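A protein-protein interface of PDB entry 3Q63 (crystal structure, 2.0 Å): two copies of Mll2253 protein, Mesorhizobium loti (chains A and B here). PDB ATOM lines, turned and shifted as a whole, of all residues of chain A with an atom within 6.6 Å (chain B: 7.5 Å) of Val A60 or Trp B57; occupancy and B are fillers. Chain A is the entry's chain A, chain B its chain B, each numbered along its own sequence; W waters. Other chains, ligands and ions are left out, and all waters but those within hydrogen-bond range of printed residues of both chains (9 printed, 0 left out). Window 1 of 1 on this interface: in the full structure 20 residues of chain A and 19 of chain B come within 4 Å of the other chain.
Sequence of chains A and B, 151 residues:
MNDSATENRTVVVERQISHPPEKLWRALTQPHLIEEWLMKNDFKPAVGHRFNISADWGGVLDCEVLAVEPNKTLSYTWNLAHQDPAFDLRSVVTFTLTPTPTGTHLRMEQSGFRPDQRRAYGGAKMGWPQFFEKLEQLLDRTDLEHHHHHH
NE of Arg A119 lies within hydrogen-bond range of OG of Ser B54 (2.9 Å). The backbone NH (N) of Ala A124 is in hydrogen-bond range of the backbone carbonyl oxygen (O) of Asp B56, 3.5 Å away. The guanidinium group of Arg A119 is in salt-bridge range of the side-chain carboxylate of Asp B56 (2.9 Å). A ring nitrogen (NE2) of His B82 lies within hydrogen-bond range of the side-chain carboxylate of Asp A62 (2.8 Å). NE1 of Trp A78 sits at hydrogen-bond distance from O of Trp B57. O of Ala B55 lies close to NH2 of Arg A119 (3.0 Å). The backbone carbonyl oxygen of Gly A123 lies close to the backbone carbonyl oxygen of Asp B56, 3.3 Å away.
N of His B82 sits at hydrogen-bond distance from OD1 of Asp B88, 3.0 Å away. The side-chain carboxylate (OD2) of Asp A62 lies within hydrogen-bond range of the side-chain amide nitrogen (ND2) of Asn A52, at 2.8 Å. NE1 of Trp A78 sits close to NE2 of Gln A110 (3.4 Å). ND2 of Asn A52 lies within hydrogen-bond range of O of Leu A61 (3.1 Å). The backbone NH of Asp A62 is in hydrogen-bond range of the backbone carbonyl oxygen of Asn A79. The backbone carbonyl oxygen (O) of Ile A53 is in hydrogen-bond range of the backbone NH (N) of Leu A61, 2.7 Å away.
Ser A54 touches Phe B87 (CB to CE1, 3.9 Å). Trp A57 touches Met B39 (CE2 to CE, 3.5 Å). Ala B55 touches Trp A57 (CB to CZ2, 3.6 Å). Trp A57 touches Trp B57 (CZ2 to CZ2, 3.3 Å). Gly A58 touches Leu B80 (O to CD1, 3.4 Å). Trp B57 touches Gly A59. N of Val A60 touches CH2 of Trp B57, at 3.9 Å. Phe B87 touches Val A60. CG of Leu A61 touches CZ3 of Trp B57 (3.6 Å). Leu A80 touches Val B60 (CD2 to CG1, 3.2 Å).
Of chain A, only Met A39, Ala A55, Trp A57, Gly A59, Val A60, Leu A61 and Trp A78 come within 4 Å of Trp B57. Of the printed residues of chain A, His B82 touches Asn A52 (3.99 Å), Val A60 (3.8 Å) and Asp A62 (2.8 Å). Printed residues of chain B within 4 Å of Gly A123: Asp B56. Of the printed residues of chain B, Asn A52 touches His B82 and Phe B87. The nearest residue of chain B that does not touch Val A60 is Gly B59 (4.6 Å). The nearest printed residue of chain B that does not touch Arg A119 is Trp B57 (5.6 Å).
Hydrophobic or aromatic side chains of chain A that line the printed part of chain B: Met A39, Ala A55, Trp A57, Val A60, Leu A61, Trp A78 and Leu A80. Along chain B the printed residues that touch a printed residue of chain A span positions 39 to 87. Among the printed residues, 26 pairs touch across the chains.
Trp B57 touches its own counterpart, Trp A57. Trp A57 touches Leu B61, and with the chains exchanged Leu A61 touches Trp B57. Gly A59 touches Trp B57, but with the chains exchanged Trp A57 does not touch Gly B59 (4.1 Å). Val A60 touches Leu B80, and with the chains exchanged Leu A80 touches Val B60. Positions printed for both chains: 39, 54, 55, 57, 58, 59, 60, 61, 80 and 81. Of the 26 pairs that touch across the chains among the printed residues, 11 have their exchanged pair printed and touching as well.
Water W6 lies within hydrogen-bond range of the side-chain carboxylate of Asp A62 (2.6 Å), a ring nitrogen (NE2) of His B82 (3.3 Å) and the backbone carbonyl oxygen of Val A60 (3.3 Å). Water W1 lies within hydrogen-bond range of the backbone carbonyl oxygen of Ala B81 (2.7 Å) and the backbone carbonyl oxygen of Ala A81 (2.7 Å). Water W5 lies within hydrogen-bond range of O of Asp B56 (2.7 Å) and O of Ala A120 (2.7 Å). Water W2 lies within hydrogen-bond range of O of Gly A123, O of Asp B56 and N of Trp B57. Water W9 lies within hydrogen-bond range of O of Ala A81 and O of Ala B81. Water W3 lies within hydrogen-bond range of NE1 of Trp A57 (3.0 Å) and NE1 of Trp B57 (3.1 Å).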
ATOM      1  N   LEU A  38     -16.227  28.780  28.189  1.00  0.00           N
ATOM      2  CA  LEU A  38     -16.211  27.368  27.818  1.00  0.00           C
ATOM      3  C   LEU A  38     -17.650  26.855  27.728  1.00  0.00           C
ATOM      4  O   LEU A  38     -18.326  27.054  26.723  1.00  0.00           O
ATOM      5  CB  LEU A  38     -15.433  26.556  28.857  1.00  0.00           C
ATOM      6  CG  LEU A  38     -14.354  25.614  28.328  1.00  0.00           C
ATOM      7  CD1 LEU A  38     -13.891  24.676  29.442  1.00  0.00           C
ATOM      8  CD2 LEU A  38     -14.896  24.806  27.164  1.00  0.00           C
ATOM      9  N   MET A  39     -18.109  26.192  28.781  1.00  0.00           N
ATOM     10  CA  MET A  39     -19.476  25.687  28.830  1.00  0.00           C
ATOM     11  C   MET A  39     -19.761  25.096  30.209  1.00  0.00           C
ATOM     12  O   MET A  39     -18.885  25.076  31.082  1.00  0.00           O
ATOM     13  CB  MET A  39     -19.701  24.630  27.738  1.00  0.00           C
ATOM     14  CG  MET A  39     -18.932  23.327  27.922  1.00  0.00           C
ATOM     15  SD  MET A  39     -19.094  22.133  26.372  1.00  0.00           S
ATOM     16  CE  MET A  39     -17.461  22.636  25.460  1.00  0.00           C
ATOM     17  N   ASN A  52     -17.425  16.898  34.882  1.00  0.00           N
ATOM     18  CA  ASN A  52     -17.768  16.867  33.472  1.00  0.00           C
ATOM     19  C   ASN A  52     -17.913  18.256  32.895  1.00  0.00           C
ATOM     20  O   ASN A  52     -18.175  19.227  33.603  1.00  0.00           O
ATOM     21  CB  ASN A  52     -19.077  16.118  33.226  1.00  0.00           C
ATOM     22  CG  ASN A  52     -19.054  14.720  33.765  1.00  0.00           C
ATOM     23  OD1 ASN A  52     -19.411  14.485  34.919  1.00  0.00           O
ATOM     24  ND2 ASN A  52     -18.625  13.770  32.936  1.00  0.00           N
ATOM     25  N   ILE A  53     -17.728  18.323  31.585  1.00  0.00           N
ATOM     26  CA  ILE A  53     -17.866  19.543  30.826  1.00  0.00           C
ATOM     27  C   ILE A  53     -18.928  19.135  29.809  1.00  0.00           C
ATOM     28  O   ILE A  53     -18.737  18.165  29.071  1.00  0.00           O
ATOM     29  CB  ILE A  53     -16.550  19.903  30.114  1.00  0.00           C
ATOM     30  CG1 ILE A  53     -15.471  20.228  31.153  1.00  0.00           C
ATOM     31  CG2 ILE A  53     -16.771  21.088  29.187  1.00  0.00           C
ATOM     32  CD1 ILE A  53     -14.110  20.535  30.553  1.00  0.00           C
ATOM     33  N   SER A  54     -20.049  19.851  29.788  1.00  0.00           N
ATOM     34  CA  SER A  54     -21.140  19.495  28.890  1.00  0.00           C
ATOM     35  C   SER A  54     -21.784  20.661  28.152  1.00  0.00           C
ATOM     36  O   SER A  54     -21.670  21.823  28.553  1.00  0.00           O
ATOM     37  CB  SER A  54     -22.222  18.739  29.671  1.00  0.00           C
ATOM     38  OG  SER A  54     -22.763  19.538  30.713  1.00  0.00           O
ATOM     39  N   ALA A  55     -22.468  20.330  27.067  1.00  0.00           N
ATOM     40  CA  ALA A  55     -23.150  21.321  26.253  1.00  0.00           C
ATOM     41  C   ALA A  55     -24.656  21.128  26.402  1.00  0.00           C
ATOM     42  O   ALA A  55     -25.114  20.035  26.712  1.00  0.00           O
ATOM     43  CB  ALA A  55     -22.741  21.160  24.789  1.00  0.00           C
ATOM     44  N   TRP A  57     -26.869  20.663  24.317  1.00  0.00           N
ATOM     45  CA  TRP A  57     -27.461  19.682  23.410  1.00  0.00           C
ATOM     46  C   TRP A  57     -27.161  18.234  23.785  1.00  0.00           C
ATOM     47  O   TRP A  57     -27.578  17.304  23.085  1.00  0.00           O
ATOM     48  CB  TRP A  57     -27.023  19.939  21.961  1.00  0.00           C
ATOM     49  CG  TRP A  57     -25.568  20.244  21.800  1.00  0.00           C
ATOM     50  CD1 TRP A  57     -24.976  21.474  21.870  1.00  0.00           C
ATOM     51  CD2 TRP A  57     -24.520  19.310  21.542  1.00  0.00           C
ATOM     52  NE1 TRP A  57     -23.624  21.363  21.666  1.00  0.00           N
ATOM     53  CE2 TRP A  57     -23.316  20.045  21.462  1.00  0.00           C
ATOM     54  CE3 TRP A  57     -24.477  17.921  21.368  1.00  0.00           C
ATOM     55  CZ2 TRP A  57     -22.083  19.436  21.215  1.00  0.00           C
ATOM     56  CZ3 TRP A  57     -23.248  17.318  21.123  1.00  0.00           C
ATOM     57  CH2 TRP A  57     -22.072  18.075  21.049  1.00  0.00           C
ATOM     58  N   GLY A  58     -26.436  18.036  24.883  1.00  0.00           N
ATOM     59  CA  GLY A  58     -26.135  16.681  25.324  1.00  0.00           C
ATOM     60  C   GLY A  58     -24.684  16.224  25.302  1.00  0.00           C
ATOM     61  O   GLY A  58     -24.316  15.319  26.049  1.00  0.00           O
ATOM     62  N   GLY A  59     -23.865  16.825  24.445  1.00  0.00           N
ATOM     63  CA  GLY A  59     -22.471  16.431  24.378  1.00  0.00           C
ATOM     64  C   GLY A  59     -21.843  16.584  25.748  1.00  0.00           C
ATOM     65  O   GLY A  59     -22.210  17.483  26.499  1.00  0.00           O
ATOM     66  N   VAL A  60     -20.898  15.715  26.083  1.00  0.00           N
ATOM     67  CA  VAL A  60     -20.260  15.773  27.389  1.00  0.00           C
ATOM     68  C   VAL A  60     -18.876  15.162  27.350  1.00  0.00           C
ATOM     69  O   VAL A  60     -18.609  14.259  26.554  1.00  0.00           O
ATOM     70  CB  VAL A  60     -21.115  15.013  28.441  1.00  0.00           C
ATOM     71  CG1 VAL A  60     -21.388  13.605  27.945  1.00  0.00           C
ATOM     72  CG2 VAL A  60     -20.404  14.970  29.785  1.00  0.00           C
ATOM     73  N   LEU A  61     -18.004  15.673  28.220  1.00  0.00           N
ATOM     74  CA  LEU A  61     -16.624  15.195  28.356  1.00  0.00           C
ATOM     75  C   LEU A  61     -16.433  14.757  29.806  1.00  0.00           C
ATOM     76  O   LEU A  61     -17.060  15.316  30.699  1.00  0.00           O
ATOM     77  CB  LEU A  61     -15.627  16.322  28.082  1.00  0.00           C
ATOM     78  CG  LEU A  61     -15.613  16.992  26.711  1.00  0.00           C
ATOM     79  CD1 LEU A  61     -14.696  18.216  26.752  1.00  0.00           C
ATOM     80  CD2 LEU A  61     -15.154  16.003  25.666  1.00  0.00           C
ATOM     81  N   ASP A  62     -15.574  13.761  30.021  1.00  0.00           N
ATOM     82  CA  ASP A  62     -15.247  13.259  31.354  1.00  0.00           C
ATOM     83  C   ASP A  62     -13.841  13.754  31.688  1.00  0.00           C
ATOM     84  O   ASP A  62     -12.907  13.546  30.906  1.00  0.00           O
ATOM     85  CB  ASP A  62     -15.253  11.733  31.386  1.00  0.00           C
ATOM     86  CG  ASP A  62     -16.653  11.144  31.272  1.00  0.00           C
ATOM     87  OD1 ASP A  62     -16.777   9.910  31.366  1.00  0.00           O
ATOM     88  OD2 ASP A  62     -17.622  11.906  31.087  1.00  0.00           O
ATOM     89  N   TRP A  78      -9.434  15.189  29.566  1.00  0.00           N
ATOM     90  CA  TRP A  78     -10.468  15.711  28.683  1.00  0.00           C
ATOM     91  C   TRP A  78     -10.738  14.528  27.769  1.00  0.00           C
ATOM     92  O   TRP A  78     -10.126  14.394  26.705  1.00  0.00           O
ATOM     93  CB  TRP A  78      -9.857  16.883  27.928  1.00  0.00           C
ATOM     94  CG  TRP A  78     -10.718  17.613  26.948  1.00  0.00           C
ATOM     95  CD1 TRP A  78     -11.122  17.180  25.714  1.00  0.00           C
ATOM     96  CD2 TRP A  78     -11.144  18.971  27.057  1.00  0.00           C
ATOM     97  NE1 TRP A  78     -11.761  18.197  25.046  1.00  0.00           N
ATOM     98  CE2 TRP A  78     -11.789  19.307  25.851  1.00  0.00           C
ATOM     99  CE3 TRP A  78     -11.036  19.943  28.066  1.00  0.00           C
ATOM    100  CZ2 TRP A  78     -12.328  20.575  25.620  1.00  0.00           C
ATOM    101  CZ3 TRP A  78     -11.568  21.193  27.840  1.00  0.00           C
ATOM    102  CH2 TRP A  78     -12.209  21.502  26.622  1.00  0.00           C
ATOM    103  N   ASN A  79     -11.650  13.667  28.211  1.00  0.00           N
ATOM    104  CA  ASN A  79     -11.973  12.439  27.495  1.00  0.00           C
ATOM    105  C   ASN A  79     -13.442  12.225  27.192  1.00  0.00           C
ATOM    106  O   ASN A  79     -14.316  12.899  27.722  1.00  0.00           O
ATOM    107  CB  ASN A  79     -11.529  11.198  28.291  1.00  0.00           C
ATOM    108  CG  ASN A  79     -10.165  11.345  28.935  1.00  0.00           C
ATOM    109  OD1 ASN A  79      -9.288  12.017  28.417  1.00  0.00           O
ATOM    110  ND2 ASN A  79      -9.981  10.678  30.075  1.00  0.00           N
ATOM    111  N   LEU A  80     -13.677  11.220  26.355  1.00  0.00           N
ATOM    112  CA  LEU A  80     -15.004  10.791  25.958  1.00  0.00           C
ATOM    113  C   LEU A  80     -14.897   9.299  25.623  1.00  0.00           C
ATOM    114  O   LEU A  80     -14.099   8.904  24.769  1.00  0.00           O
ATOM    115  CB  LEU A  80     -15.480  11.576  24.734  1.00  0.00           C
ATOM    116  CG  LEU A  80     -16.752  11.067  24.056  1.00  0.00           C
ATOM    117  CD1 LEU A  80     -17.871  10.920  25.079  1.00  0.00           C
ATOM    118  CD2 LEU A  80     -17.154  12.036  22.961  1.00  0.00           C
ATOM    119  N   ALA A  81     -15.665   8.464  26.318  1.00  0.00           N
ATOM    120  CA  ALA A  81     -15.645   7.031  26.037  1.00  0.00           C
ATOM    121  C   ALA A  81     -16.632   6.784  24.902  1.00  0.00           C
ATOM    122  O   ALA A  81     -17.789   7.184  24.989  1.00  0.00           O
ATOM    123  CB  ALA A  81     -16.061   6.240  27.271  1.00  0.00           C
ATOM    124  N   LEU A  89     -11.900   9.611  22.663  1.00  0.00           N
ATOM    125  CA  LEU A  89     -10.837  10.528  23.026  1.00  0.00           C
ATOM    126  C   LEU A  89     -10.281  10.422  24.443  1.00  0.00           C
ATOM    127  O   LEU A  89     -11.023  10.321  25.419  1.00  0.00           O
ATOM    128  CB  LEU A  89     -11.332  11.957  22.798  1.00  0.00           C
ATOM    129  CG  LEU A  89     -10.349  13.115  22.970  1.00  0.00           C
ATOM    130  CD1 LEU A  89      -9.206  12.973  21.957  1.00  0.00           C
ATOM    131  CD2 LEU A  89     -11.084  14.437  22.740  1.00  0.00           C
ATOM    132  N   GLN A 110      -2.884  20.598  24.703  1.00  0.00           N
ATOM    133  CA  GLN A 110      -3.791  19.458  24.753  1.00  0.00           C
ATOM    134  C   GLN A 110      -3.128  18.294  24.032  1.00  0.00           C
ATOM    135  O   GLN A 110      -2.891  18.354  22.820  1.00  0.00           O
ATOM    136  CB  GLN A 110      -5.136  19.766  24.098  1.00  0.00           C
ATOM    137  CG  GLN A 110      -6.073  18.561  24.105  1.00  0.00           C
ATOM    138  CD  GLN A 110      -7.506  18.920  23.798  1.00  0.00           C
ATOM    139  OE1 GLN A 110      -7.776  19.858  23.048  1.00  0.00           O
ATOM    140  NE2 GLN A 110      -8.440  18.160  24.358  1.00  0.00           N
ATOM    141  N   ARG A 119     -10.713  14.464  13.310  1.00  0.00           N
ATOM    142  CA  ARG A 119     -11.867  15.279  13.659  1.00  0.00           C
ATOM    143  C   ARG A 119     -11.613  16.029  14.974  1.00  0.00           C
ATOM    144  O   ARG A 119     -11.760  17.247  15.041  1.00  0.00           O
ATOM    145  CB  ARG A 119     -13.107  14.398  13.815  1.00  0.00           C
ATOM    146  CG  ARG A 119     -14.288  15.105  14.475  1.00  0.00           C
ATOM    147  CD  ARG A 119     -14.961  16.025  13.500  1.00  0.00           C
ATOM    148  NE  ARG A 119     -16.012  16.855  14.103  1.00  0.00           N
ATOM    149  CZ  ARG A 119     -15.811  18.052  14.644  1.00  0.00           C
ATOM    150  NH1 ARG A 119     -14.587  18.572  14.672  1.00  0.00           N
ATOM    151  NH2 ARG A 119     -16.840  18.744  15.118  1.00  0.00           N
ATOM    152  N   ALA A 120     -11.240  15.288  16.013  1.00  0.00           N
ATOM    153  CA  ALA A 120     -10.973  15.879  17.319  1.00  0.00           C
ATOM    154  C   ALA A 120      -9.742  16.773  17.256  1.00  0.00           C
ATOM    155  O   ALA A 120      -9.729  17.872  17.814  1.00  0.00           O
ATOM    156  CB  ALA A 120     -10.776  14.782  18.360  1.00  0.00           C
ATOM    157  N   GLY A 123     -10.699  19.867  15.288  1.00  0.00           N
ATOM    158  CA  GLY A 123     -11.660  20.641  16.052  1.00  0.00           C
ATOM    159  C   GLY A 123     -11.000  21.399  17.189  1.00  0.00           C
ATOM    160  O   GLY A 123     -11.452  22.477  17.575  1.00  0.00           O
ATOM    161  N   ALA A 124      -9.921  20.834  17.719  1.00  0.00           N
ATOM    162  CA  ALA A 124      -9.186  21.445  18.822  1.00  0.00           C
ATOM    163  C   ALA A 124      -8.401  22.667  18.359  1.00  0.00           C
ATOM    164  O   ALA A 124      -8.363  23.681  19.051  1.00  0.00           O
ATOM    165  CB  ALA A 124      -8.232  20.413  19.444  1.00  0.00           C
ATOM    166  N   GLY A 127     -11.249  25.212  17.639  1.00  0.00           N
ATOM    167  CA  GLY A 127     -11.991  25.664  18.806  1.00  0.00           C
ATOM    168  C   GLY A 127     -11.250  26.408  19.899  1.00  0.00           C
ATOM    169  O   GLY A 127     -11.782  27.361  20.451  1.00  0.00           O
ATOM    170  N   PHE A 131     -12.234  29.672  22.050  1.00  0.00           N
ATOM    171  CA  PHE A 131     -12.404  29.598  23.504  1.00  0.00           C
ATOM    172  C   PHE A 131     -11.576  30.689  24.164  1.00  0.00           C
ATOM    173  O   PHE A 131     -12.016  31.326  25.124  1.00  0.00           O
ATOM    174  CB  PHE A 131     -11.966  28.228  24.028  1.00  0.00           C
ATOM    175  CG  PHE A 131     -12.974  27.132  23.785  1.00  0.00           C
ATOM    176  CD1 PHE A 131     -12.566  25.804  23.681  1.00  0.00           C
ATOM    177  CD2 PHE A 131     -14.329  27.425  23.665  1.00  0.00           C
ATOM    178  CE1 PHE A 131     -13.492  24.784  23.459  1.00  0.00           C
ATOM    179  CE2 PHE A 131     -15.263  26.416  23.445  1.00  0.00           C
ATOM    180  CZ  PHE A 131     -14.844  25.093  23.340  1.00  0.00           C
ATOM    181  N   MET B  39     -24.027  21.381  13.523  1.00  0.00           N
ATOM    182  CA  MET B  39     -22.605  21.056  13.628  1.00  0.00           C
ATOM    183  C   MET B  39     -22.249  19.889  12.713  1.00  0.00           C
ATOM    184  O   MET B  39     -23.116  19.319  12.048  1.00  0.00           O
ATOM    185  CB  MET B  39     -22.220  20.722  15.078  1.00  0.00           C
ATOM    186  CG  MET B  39     -22.769  19.403  15.599  1.00  0.00           C
ATOM    187  SD  MET B  39     -22.566  19.196  17.531  1.00  0.00           S
ATOM    188  CE  MET B  39     -24.227  20.003  18.121  1.00  0.00           C
ATOM    189  N   SER B  54     -21.087  15.714  15.653  1.00  0.00           N
ATOM    190  CA  SER B  54     -19.984  15.983  16.571  1.00  0.00           C
ATOM    191  C   SER B  54     -19.518  17.433  16.605  1.00  0.00           C
ATOM    192  O   SER B  54     -19.635  18.173  15.622  1.00  0.00           O
ATOM    193  CB  SER B  54     -18.796  15.070  16.233  1.00  0.00           C
ATOM    194  OG  SER B  54     -18.291  15.340  14.933  1.00  0.00           O
ATOM    195  N   ALA B  55     -18.969  17.821  17.753  1.00  0.00           N
ATOM    196  CA  ALA B  55     -18.484  19.177  17.981  1.00  0.00           C
ATOM    197  C   ALA B  55     -16.964  19.269  17.900  1.00  0.00           C
ATOM    198  O   ALA B  55     -16.267  18.264  18.030  1.00  0.00           O
ATOM    199  CB  ALA B  55     -18.955  19.653  19.352  1.00  0.00           C
ATOM    200  N   ASP B  56     -16.441  20.477  17.716  1.00  0.00           N
ATOM    201  CA  ASP B  56     -14.992  20.640  17.618  1.00  0.00           C
ATOM    202  C   ASP B  56     -14.246  20.313  18.910  1.00  0.00           C
ATOM    203  O   ASP B  56     -13.081  19.927  18.864  1.00  0.00           O
ATOM    204  CB  ASP B  56     -14.627  22.064  17.181  1.00  0.00           C
ATOM    205  CG  ASP B  56     -15.021  22.355  15.738  1.00  0.00           C
ATOM    206  OD1 ASP B  56     -15.130  21.399  14.938  1.00  0.00           O
ATOM    207  OD2 ASP B  56     -15.201  23.542  15.408  1.00  0.00           O
ATOM    208  N   TRP B  57     -14.916  20.454  20.050  1.00  0.00           N
ATOM    209  CA  TRP B  57     -14.288  20.193  21.344  1.00  0.00           C
ATOM    210  C   TRP B  57     -14.279  18.727  21.785  1.00  0.00           C
ATOM    211  O   TRP B  57     -13.788  18.404  22.871  1.00  0.00           O
ATOM    212  CB  TRP B  57     -14.944  21.052  22.427  1.00  0.00           C
ATOM    213  CG  TRP B  57     -16.444  21.039  22.417  1.00  0.00           C
ATOM    214  CD1 TRP B  57     -17.266  21.910  21.766  1.00  0.00           C
ATOM    215  CD2 TRP B  57     -17.294  20.162  23.160  1.00  0.00           C
ATOM    216  NE1 TRP B  57     -18.577  21.639  22.067  1.00  0.00           N
ATOM    217  CE2 TRP B  57     -18.623  20.567  22.920  1.00  0.00           C
ATOM    218  CE3 TRP B  57     -17.063  19.073  24.010  1.00  0.00           C
ATOM    219  CZ2 TRP B  57     -19.719  19.922  23.500  1.00  0.00           C
ATOM    220  CZ3 TRP B  57     -18.153  18.433  24.586  1.00  0.00           C
ATOM    221  CH2 TRP B  57     -19.463  18.860  24.328  1.00  0.00           C
ATOM    222  N   GLY B  58     -14.838  17.851  20.951  1.00  0.00           N
ATOM    223  CA  GLY B  58     -14.851  16.432  21.260  1.00  0.00           C
ATOM    224  C   GLY B  58     -16.196  15.765  21.511  1.00  0.00           C
ATOM    225  O   GLY B  58     -16.296  14.550  21.398  1.00  0.00           O
ATOM    226  N   GLY B  59     -17.222  16.539  21.851  1.00  0.00           N
ATOM    227  CA  GLY B  59     -18.526  15.954  22.120  1.00  0.00           C
ATOM    228  C   GLY B  59     -19.106  15.296  20.887  1.00  0.00           C
ATOM    229  O   GLY B  59     -18.865  15.753  19.769  1.00  0.00           O
ATOM    230  N   VAL B  60     -19.875  14.229  21.078  1.00  0.00           N
ATOM    231  CA  VAL B  60     -20.461  13.521  19.941  1.00  0.00           C
ATOM    232  C   VAL B  60     -21.766  12.839  20.310  1.00  0.00           C
ATOM    233  O   VAL B  60     -21.939  12.383  21.432  1.00  0.00           O
ATOM    234  CB  VAL B  60     -19.479  12.457  19.386  1.00  0.00           C
ATOM    235  CG1 VAL B  60     -19.105  11.484  20.466  1.00  0.00           C
ATOM    236  CG2 VAL B  60     -20.097  11.726  18.201  1.00  0.00           C
ATOM    237  N   LEU B  61     -22.680  12.791  19.349  1.00  0.00           N
ATOM    238  CA  LEU B  61     -23.972  12.155  19.527  1.00  0.00           C
ATOM    239  C   LEU B  61     -24.102  11.058  18.484  1.00  0.00           C
ATOM    240  O   LEU B  61     -23.568  11.181  17.379  1.00  0.00           O
ATOM    241  CB  LEU B  61     -25.105  13.164  19.324  1.00  0.00           C
ATOM    242  CG  LEU B  61     -25.336  14.164  20.451  1.00  0.00           C
ATOM    243  CD1 LEU B  61     -26.318  15.205  19.991  1.00  0.00           C
ATOM    244  CD2 LEU B  61     -25.832  13.440  21.683  1.00  0.00           C
ATOM    245  N   LEU B  80     -26.624   9.402  23.425  1.00  0.00           N
ATOM    246  CA  LEU B  80     -25.256   9.462  23.910  1.00  0.00           C
ATOM    247  C   LEU B  80     -25.153   8.456  25.056  1.00  0.00           C
ATOM    248  O   LEU B  80     -25.769   8.630  26.107  1.00  0.00           O
ATOM    249  CB  LEU B  80     -24.945  10.893  24.361  1.00  0.00           C
ATOM    250  CG  LEU B  80     -23.491  11.260  24.614  1.00  0.00           C
ATOM    251  CD1 LEU B  80     -23.240  12.706  24.205  1.00  0.00           C
ATOM    252  CD2 LEU B  80     -23.180  11.042  26.079  1.00  0.00           C
ATOM    253  N   ALA B  81     -24.407   7.380  24.830  1.00  0.00           N
ATOM    254  CA  ALA B  81     -24.239   6.353  25.851  1.00  0.00           C
ATOM    255  C   ALA B  81     -23.218   6.821  26.881  1.00  0.00           C
ATOM    256  O   ALA B  81     -22.073   7.127  26.542  1.00  0.00           O
ATOM    257  CB  ALA B  81     -23.783   5.046  25.211  1.00  0.00           C
ATOM    258  N   HIS B  82     -23.636   6.888  28.141  1.00  0.00           N
ATOM    259  CA  HIS B  82     -22.741   7.332  29.208  1.00  0.00           C
ATOM    260  C   HIS B  82     -23.014   6.542  30.477  1.00  0.00           C
ATOM    261  O   HIS B  82     -24.160   6.202  30.783  1.00  0.00           O
ATOM    262  CB  HIS B  82     -22.927   8.832  29.466  1.00  0.00           C
ATOM    263  CG  HIS B  82     -21.803   9.470  30.227  1.00  0.00           C
ATOM    264  ND1 HIS B  82     -21.637   9.317  31.588  1.00  0.00           N
ATOM    265  CD2 HIS B  82     -20.813  10.302  29.822  1.00  0.00           C
ATOM    266  CE1 HIS B  82     -20.600  10.033  31.989  1.00  0.00           C
ATOM    267  NE2 HIS B  82     -20.083  10.641  30.935  1.00  0.00           N
ATOM    268  N   PHE B  87     -26.254  11.693  32.160  1.00  0.00           N
ATOM    269  CA  PHE B  87     -25.796  12.025  30.815  1.00  0.00           C
ATOM    270  C   PHE B  87     -26.157  10.981  29.763  1.00  0.00           C
ATOM    271  O   PHE B  87     -26.122  11.265  28.564  1.00  0.00           O
ATOM    272  CB  PHE B  87     -24.280  12.238  30.822  1.00  0.00           C
ATOM    273  CG  PHE B  87     -23.848  13.457  31.580  1.00  0.00           C
ATOM    274  CD1 PHE B  87     -24.140  14.724  31.099  1.00  0.00           C
ATOM    275  CD2 PHE B  87     -23.170  13.341  32.787  1.00  0.00           C
ATOM    276  CE1 PHE B  87     -23.763  15.863  31.810  1.00  0.00           C
ATOM    277  CE2 PHE B  87     -22.789  14.472  33.505  1.00  0.00           C
ATOM    278  CZ  PHE B  87     -23.087  15.734  33.016  1.00  0.00           C
ATOM    279  N   ASP B  88     -26.496   9.774  30.207  1.00  0.00           N
ATOM    280  CA  ASP B  88     -26.869   8.698  29.293  1.00  0.00           C
ATOM    281  C   ASP B  88     -28.168   9.103  28.586  1.00  0.00           C
ATOM    282  O   ASP B  88     -29.262   8.757  29.026  1.00  0.00           O
ATOM    283  CB  ASP B  88     -27.064   7.404  30.082  1.00  0.00           C
ATOM    284  CG  ASP B  88     -27.281   6.201  29.191  1.00  0.00           C
ATOM    285  OD1 ASP B  88     -26.437   5.952  28.304  1.00  0.00           O
ATOM    286  OD2 ASP B  88     -28.294   5.499  29.388  1.00  0.00           O
HETATM  287  O   HOH W   1     -20.426   6.978  24.448  1.00  0.00           O
HETATM  288  O   HOH W   2     -12.725  22.958  19.983  1.00  0.00           O
HETATM  289  O   HOH W   3     -21.231  23.059  21.332  1.00  0.00           O
HETATM  290  O   HOH W   4     -19.044  21.242  14.113  1.00  0.00           O
HETATM  291  O   HOH W   5     -11.200  18.381  20.045  1.00  0.00           O
HETATM  292  O   HOH W   6     -18.130  11.697  28.534  1.00  0.00           O
HETATM  293  O   HOH W   7     -20.203  13.406  24.215  1.00  0.00           O
HETATM  294  O   HOH W   8     -26.082  13.972  27.623  1.00  0.00           O
HETATM  295  O   HOH W   9     -19.369   7.634  27.301  1.00  0.00           O
